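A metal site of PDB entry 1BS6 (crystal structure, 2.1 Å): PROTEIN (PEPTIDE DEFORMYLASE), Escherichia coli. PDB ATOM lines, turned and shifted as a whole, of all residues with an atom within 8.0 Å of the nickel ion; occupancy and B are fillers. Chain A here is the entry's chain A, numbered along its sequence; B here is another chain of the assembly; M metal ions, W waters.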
ATOM      1  N   VAL A   5     -11.006   9.060 -25.632  1.00  0.00           N
ATOM      2  CA  VAL A   5     -11.695   9.588 -24.448  1.00  0.00           C
ATOM      3  C   VAL A   5     -10.697  10.110 -23.429  1.00  0.00           C
ATOM      4  O   VAL A   5      -9.777   9.388 -22.997  1.00  0.00           O
ATOM      5  CB  VAL A   5     -12.559   8.481 -23.779  1.00  0.00           C
ATOM      6  CG1 VAL A   5     -13.241   9.023 -22.532  1.00  0.00           C
ATOM      7  CG2 VAL A   5     -13.611   7.957 -24.750  1.00  0.00           C
ATOM      8  N   LEU A  13     -11.449  18.260 -19.409  1.00  0.00           N
ATOM      9  CA  LEU A  13     -12.706  17.747 -18.871  1.00  0.00           C
ATOM     10  C   LEU A  13     -13.495  18.816 -18.121  1.00  0.00           C
ATOM     11  O   LEU A  13     -14.662  18.633 -17.839  1.00  0.00           O
ATOM     12  CB  LEU A  13     -12.415  16.572 -17.919  1.00  0.00           C
ATOM     13  CG  LEU A  13     -12.660  15.116 -18.323  1.00  0.00           C
ATOM     14  CD1 LEU A  13     -13.151  14.991 -19.747  1.00  0.00           C
ATOM     15  CD2 LEU A  13     -11.364  14.340 -18.077  1.00  0.00           C
ATOM     16  N   GLY A  45     -23.849   6.147 -22.633  1.00  0.00           N
ATOM     17  CA  GLY A  45     -23.904   7.567 -22.931  1.00  0.00           C
ATOM     18  C   GLY A  45     -22.518   8.175 -23.105  1.00  0.00           C
ATOM     19  O   GLY A  45     -21.540   7.652 -22.578  1.00  0.00           O
ATOM     20  N   LEU A  46     -22.435   9.239 -23.895  1.00  0.00           N
ATOM     21  CA  LEU A  46     -21.185   9.957 -24.117  1.00  0.00           C
ATOM     22  C   LEU A  46     -21.504  11.437 -24.400  1.00  0.00           C
ATOM     23  O   LEU A  46     -22.486  11.732 -25.075  1.00  0.00           O
ATOM     24  CB  LEU A  46     -20.438   9.336 -25.305  1.00  0.00           C
ATOM     25  CG  LEU A  46     -19.075   9.848 -25.749  1.00  0.00           C
ATOM     26  CD1 LEU A  46     -18.008   9.484 -24.753  1.00  0.00           C
ATOM     27  CD2 LEU A  46     -18.737   9.209 -27.067  1.00  0.00           C
ATOM     28  N   ALA A  47     -20.804  12.332 -23.717  1.00  0.00           N
ATOM     29  CA  ALA A  47     -20.870  13.778 -23.947  1.00  0.00           C
ATOM     30  C   ALA A  47     -19.698  14.193 -24.817  1.00  0.00           C
ATOM     31  O   ALA A  47     -18.581  13.666 -24.628  1.00  0.00           O
ATOM     32  CB  ALA A  47     -20.805  14.528 -22.623  1.00  0.00           C
ATOM     33  N   GLN A  50     -16.016  14.852 -23.374  1.00  0.00           N
ATOM     34  CA  GLN A  50     -15.104  13.761 -22.985  1.00  0.00           C
ATOM     35  C   GLN A  50     -14.216  13.356 -24.166  1.00  0.00           C
ATOM     36  O   GLN A  50     -13.302  12.534 -24.014  1.00  0.00           O
ATOM     37  CB  GLN A  50     -15.867  12.510 -22.541  1.00  0.00           C
ATOM     38  CG  GLN A  50     -16.936  12.714 -21.515  1.00  0.00           C
ATOM     39  CD  GLN A  50     -17.682  11.440 -21.230  1.00  0.00           C
ATOM     40  OE1 GLN A  50     -18.856  11.316 -21.565  1.00  0.00           O
ATOM     41  NE2 GLN A  50     -16.991  10.454 -20.676  1.00  0.00           N
ATOM     42  N   GLU A  88     -22.870   4.888 -10.379  1.00  0.00           N
ATOM     43  CA  GLU A  88     -22.519   5.355 -11.723  1.00  0.00           C
ATOM     44  C   GLU A  88     -21.103   4.972 -12.099  1.00  0.00           C
ATOM     45  O   GLU A  88     -20.212   5.036 -11.266  1.00  0.00           O
ATOM     46  CB  GLU A  88     -22.676   6.877 -11.800  1.00  0.00           C
ATOM     47  CG  GLU A  88     -24.116   7.298 -11.868  1.00  0.00           C
ATOM     48  CD  GLU A  88     -24.304   8.788 -12.021  1.00  0.00           C
ATOM     49  OE1 GLU A  88     -23.436   9.484 -12.581  1.00  0.00           O
ATOM     50  OE2 GLU A  88     -25.368   9.274 -11.602  1.00  0.00           O
ATOM     51  N   GLY A  89     -20.873   4.620 -13.355  1.00  0.00           N
ATOM     52  CA  GLY A  89     -19.522   4.633 -13.856  1.00  0.00           C
ATOM     53  C   GLY A  89     -19.317   5.751 -14.877  1.00  0.00           C
ATOM     54  O   GLY A  89     -20.263   6.191 -15.531  1.00  0.00           O
ATOM     55  N   CYS A  90     -18.060   6.112 -15.102  1.00  0.00           N
ATOM     56  CA  CYS A  90     -17.707   7.131 -16.097  1.00  0.00           C
ATOM     57  C   CYS A  90     -16.496   6.653 -16.941  1.00  0.00           C
ATOM     58  O   CYS A  90     -15.488   6.175 -16.385  1.00  0.00           O
ATOM     59  CB  CYS A  90     -17.373   8.458 -15.381  1.00  0.00           C
ATOM     60  SG  CYS A  90     -17.090   9.899 -16.404  1.00  0.00           S
ATOM     61  N   LEU A  91     -16.606   6.740 -18.261  1.00  0.00           N
ATOM     62  CA  LEU A  91     -15.540   6.307 -19.162  1.00  0.00           C
ATOM     63  C   LEU A  91     -14.278   7.120 -18.936  1.00  0.00           C
ATOM     64  O   LEU A  91     -13.195   6.711 -19.316  1.00  0.00           O
ATOM     65  CB  LEU A  91     -15.947   6.444 -20.631  1.00  0.00           C
ATOM     66  CG  LEU A  91     -17.056   5.593 -21.274  1.00  0.00           C
ATOM     67  CD1 LEU A  91     -18.316   5.655 -20.423  1.00  0.00           C
ATOM     68  CD2 LEU A  91     -17.360   6.129 -22.677  1.00  0.00           C
ATOM     69  N   SER A  92     -14.416   8.291 -18.320  1.00  0.00           N
ATOM     70  CA  SER A  92     -13.292   9.200 -18.141  1.00  0.00           C
ATOM     71  C   SER A  92     -12.680   9.014 -16.749  1.00  0.00           C
ATOM     72  O   SER A  92     -11.586   9.519 -16.441  1.00  0.00           O
ATOM     73  CB  SER A  92     -13.767  10.645 -18.352  1.00  0.00           C
ATOM     74  OG  SER A  92     -14.570  10.764 -19.523  1.00  0.00           O
ATOM     75  N   ILE A  93     -13.368   8.241 -15.925  1.00  0.00           N
ATOM     76  CA  ILE A  93     -12.889   7.896 -14.588  1.00  0.00           C
ATOM     77  C   ILE A  93     -12.846   6.374 -14.443  1.00  0.00           C
ATOM     78  O   ILE A  93     -13.746   5.774 -13.837  1.00  0.00           O
ATOM     79  CB  ILE A  93     -13.800   8.486 -13.497  1.00  0.00           C
ATOM     80  CG1 ILE A  93     -13.909  10.009 -13.652  1.00  0.00           C
ATOM     81  CG2 ILE A  93     -13.251   8.148 -12.126  1.00  0.00           C
ATOM     82  CD1 ILE A  93     -14.992  10.648 -12.800  1.00  0.00           C
ATOM     83  N   ARG A 102     -29.387  12.113  -7.822  1.00  0.00           N
ATOM     84  CA  ARG A 102     -29.945  12.623  -9.061  1.00  0.00           C
ATOM     85  C   ARG A 102     -31.426  12.872  -8.875  1.00  0.00           C
ATOM     86  O   ARG A 102     -32.016  12.362  -7.939  1.00  0.00           O
ATOM     87  CB  ARG A 102     -29.766  11.604 -10.195  1.00  0.00           C
ATOM     88  CG  ARG A 102     -28.324  11.245 -10.518  1.00  0.00           C
ATOM     89  CD  ARG A 102     -27.588  12.404 -11.164  1.00  0.00           C
ATOM     90  NE  ARG A 102     -26.237  12.035 -11.533  1.00  0.00           N
ATOM     91  CZ  ARG A 102     -25.289  12.890 -11.909  1.00  0.00           C
ATOM     92  NH1 ARG A 102     -25.542  14.188 -11.954  1.00  0.00           N
ATOM     93  NH2 ARG A 102     -24.089  12.449 -12.222  1.00  0.00           N
ATOM     94  N   CYS A 129     -28.963   9.124 -16.581  1.00  0.00           N
ATOM     95  CA  CYS A 129     -28.025   9.210 -17.679  1.00  0.00           C
ATOM     96  C   CYS A 129     -27.980  10.591 -18.345  1.00  0.00           C
ATOM     97  O   CYS A 129     -26.904  11.115 -18.618  1.00  0.00           O
ATOM     98  CB  CYS A 129     -28.353   8.156 -18.708  1.00  0.00           C
ATOM     99  SG  CYS A 129     -27.048   8.011 -19.900  1.00  0.00           S
ATOM    100  N   HIS A 132     -26.178  12.914 -15.977  1.00  0.00           N
ATOM    101  CA  HIS A 132     -24.742  12.630 -15.950  1.00  0.00           C
ATOM    102  C   HIS A 132     -24.051  13.270 -17.163  1.00  0.00           C
ATOM    103  O   HIS A 132     -22.926  13.763 -17.072  1.00  0.00           O
ATOM    104  CB  HIS A 132     -24.541  11.104 -15.957  1.00  0.00           C
ATOM    105  CG  HIS A 132     -23.101  10.664 -16.057  1.00  0.00           C
ATOM    106  ND1 HIS A 132     -22.436  10.059 -15.015  1.00  0.00           N
ATOM    107  CD2 HIS A 132     -22.249  10.662 -17.105  1.00  0.00           C
ATOM    108  CE1 HIS A 132     -21.220   9.721 -15.400  1.00  0.00           C
ATOM    109  NE2 HIS A 132     -21.081  10.072 -16.673  1.00  0.00           N
ATOM    110  N   GLU A 133     -24.700  13.201 -18.321  1.00  0.00           N
ATOM    111  CA  GLU A 133     -24.050  13.618 -19.551  1.00  0.00           C
ATOM    112  C   GLU A 133     -24.104  15.137 -19.615  1.00  0.00           C
ATOM    113  O   GLU A 133     -23.134  15.784 -20.010  1.00  0.00           O
ATOM    114  CB  GLU A 133     -24.748  13.028 -20.796  1.00  0.00           C
ATOM    115  CG  GLU A 133     -24.796  11.491 -20.929  1.00  0.00           C
ATOM    116  CD  GLU A 133     -23.492  10.801 -20.646  1.00  0.00           C
ATOM    117  OE1 GLU A 133     -22.407  11.397 -20.834  1.00  0.00           O
ATOM    118  OE2 GLU A 133     -23.548   9.641 -20.221  1.00  0.00           O
ATOM    119  N   ASP A 135     -24.119  17.217 -17.197  1.00  0.00           N
ATOM    120  CA  ASP A 135     -23.062  17.687 -16.293  1.00  0.00           C
ATOM    121  C   ASP A 135     -21.730  17.822 -17.008  1.00  0.00           C
ATOM    122  O   ASP A 135     -20.965  18.750 -16.739  1.00  0.00           O
ATOM    123  CB  ASP A 135     -22.893  16.697 -15.125  1.00  0.00           C
ATOM    124  CG  ASP A 135     -23.749  17.046 -13.928  1.00  0.00           C
ATOM    125  OD1 ASP A 135     -24.556  18.005 -13.980  1.00  0.00           O
ATOM    126  OD2 ASP A 135     -23.597  16.354 -12.906  1.00  0.00           O
ATOM    127  N   HIS A 136     -21.394  16.840 -17.844  1.00  0.00           N
ATOM    128  CA  HIS A 136     -20.128  16.859 -18.582  1.00  0.00           C
ATOM    129  C   HIS A 136     -19.967  18.146 -19.352  1.00  0.00           C
ATOM    130  O   HIS A 136     -18.866  18.691 -19.398  1.00  0.00           O
ATOM    131  CB  HIS A 136     -20.068  15.719 -19.569  1.00  0.00           C
ATOM    132  CG  HIS A 136     -19.560  14.456 -18.969  1.00  0.00           C
ATOM    133  ND1 HIS A 136     -18.393  14.389 -18.240  1.00  0.00           N
ATOM    134  CD2 HIS A 136     -20.071  13.194 -18.988  1.00  0.00           C
ATOM    135  CE1 HIS A 136     -18.194  13.134 -17.852  1.00  0.00           C
ATOM    136  NE2 HIS A 136     -19.193  12.394 -18.301  1.00  0.00           N
ATOM    137  N   LYS A 140     -18.640  19.354 -15.118  1.00  0.00           N
ATOM    138  CA  LYS A 140     -18.800  18.623 -13.866  1.00  0.00           C
ATOM    139  C   LYS A 140     -18.637  17.102 -14.032  1.00  0.00           C
ATOM    140  O   LYS A 140     -19.164  16.510 -14.982  1.00  0.00           O
ATOM    141  CB  LYS A 140     -20.176  18.865 -13.274  1.00  0.00           C
ATOM    142  CG  LYS A 140     -20.451  20.273 -12.856  1.00  0.00           C
ATOM    143  CD  LYS A 140     -21.587  20.288 -11.844  1.00  0.00           C
ATOM    144  CE  LYS A 140     -21.435  19.125 -10.850  1.00  0.00           C
ATOM    145  NZ  LYS A 140     -22.178  19.383  -9.589  1.00  0.00           N
ATOM    146  N   LEU A 141     -18.040  16.460 -13.028  1.00  0.00           N
ATOM    147  CA  LEU A 141     -17.878  15.008 -13.029  1.00  0.00           C
ATOM    148  C   LEU A 141     -18.640  14.457 -11.831  1.00  0.00           C
ATOM    149  O   LEU A 141     -18.970  15.215 -10.916  1.00  0.00           O
ATOM    150  CB  LEU A 141     -16.384  14.648 -12.937  1.00  0.00           C
ATOM    151  CG  LEU A 141     -15.508  15.336 -14.006  1.00  0.00           C
ATOM    152  CD1 LEU A 141     -14.054  15.157 -13.681  1.00  0.00           C
ATOM    153  CD2 LEU A 141     -15.809  14.776 -15.359  1.00  0.00           C
ATOM    154  N   PHE A 142     -18.958  13.166 -11.818  1.00  0.00           N
ATOM    155  CA  PHE A 142     -19.774  12.618 -10.728  1.00  0.00           C
ATOM    156  C   PHE A 142     -19.030  12.611  -9.386  1.00  0.00           C
ATOM    157  O   PHE A 142     -19.648  12.742  -8.321  1.00  0.00           O
ATOM    158  CB  PHE A 142     -20.331  11.227 -11.080  1.00  0.00           C
ATOM    159  CG  PHE A 142     -19.363  10.089 -10.912  1.00  0.00           C
ATOM    160  CD1 PHE A 142     -19.042   9.618  -9.644  1.00  0.00           C
ATOM    161  CD2 PHE A 142     -18.818   9.458 -12.014  1.00  0.00           C
ATOM    162  CE1 PHE A 142     -18.174   8.539  -9.485  1.00  0.00           C
ATOM    163  CE2 PHE A 142     -17.949   8.357 -11.866  1.00  0.00           C
ATOM    164  CZ  PHE A 142     -17.626   7.901 -10.581  1.00  0.00           C
ATOM    165  N   MET B   1     -21.747   7.732 -19.781  1.00  0.00           N
ATOM    166  CA  MET B   1     -21.903   6.897 -18.577  1.00  0.00           C
ATOM    167  C   MET B   1     -21.589   5.418 -18.885  1.00  0.00           C
ATOM    168  O   MET B   1     -21.772   4.967 -20.014  1.00  0.00           O
ATOM    169  CB  MET B   1     -23.321   7.045 -18.035  1.00  0.00           C
ATOM    170  CG  MET B   1     -23.615   6.184 -16.851  1.00  0.00           C
ATOM    171  SD  MET B   1     -24.943   6.773 -15.852  1.00  0.00           S
ATOM    172  CE  MET B   1     -26.286   5.917 -16.522  1.00  0.00           C
ATOM    173  N   ALA B   2     -20.975   4.728 -17.913  1.00  0.00           N
ATOM    174  CA  ALA B   2     -20.868   3.266 -17.940  1.00  0.00           C
ATOM    175  C   ALA B   2     -21.818   2.587 -16.917  1.00  0.00           C
ATOM    176  O   ALA B   2     -21.753   2.856 -15.695  1.00  0.00           O
ATOM    177  CB  ALA B   2     -19.420   2.833 -17.680  1.00  0.00           C
HETATM  178 NI    NI M   1     -19.134  10.140 -17.668  1.00  0.00          NI
HETATM  179  O   HOH W   1     -18.783   8.223 -18.889  1.00  0.00           O
HETATM  180  O   HOH W   2     -20.419  10.143 -19.417  1.00  0.00           O
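The side-chain amide nitrogen (NE2) of Gln 50 sits at hydrogen-bond distance from the side-chain hydroxyl (OG) of Ser 92 (2.7 Å). A ring nitrogen (NE2) of His 136 lies close to the side-chain amide oxygen of Gln 50 (3.5 Å). The backbone NH (N) of Ala 47 sits at hydrogen-bond distance from the side-chain amide oxygen (OE1) of Gln 50, at 3.1 Å. ND1 of His 132 sits at hydrogen-bond distance from OE1 of Glu 88 (2.7 Å). The backbone NH of Ser 92 sits close to the side-chain sulfur of Cys 90 (3.7 Å).
Merely in contact with the nickel ion: Gln 50. The nearest printed residue that does not touch the nickel ion is Met 1 of chain B (4.1 Å).
The nickel ion is bound by water W2 (2.2 Å), a ring nitrogen (NE2) of His 132 (2.2 Å), water W1 (2.3 Å), a ring nitrogen (NE2) of His 136 (2.3 Å) and the side-chain sulfur of Cys 90 (2.4 Å). The nickel ion has five donor atoms within binding distance.
Water W2 lies within hydrogen-bond range of the side-chain carboxylate of Glu 133 (2.7 Å), the backbone NH of Met 1 of chain B (2.8 Å) and the side-chain amide oxygen of Gln 50 (2.9 Å).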
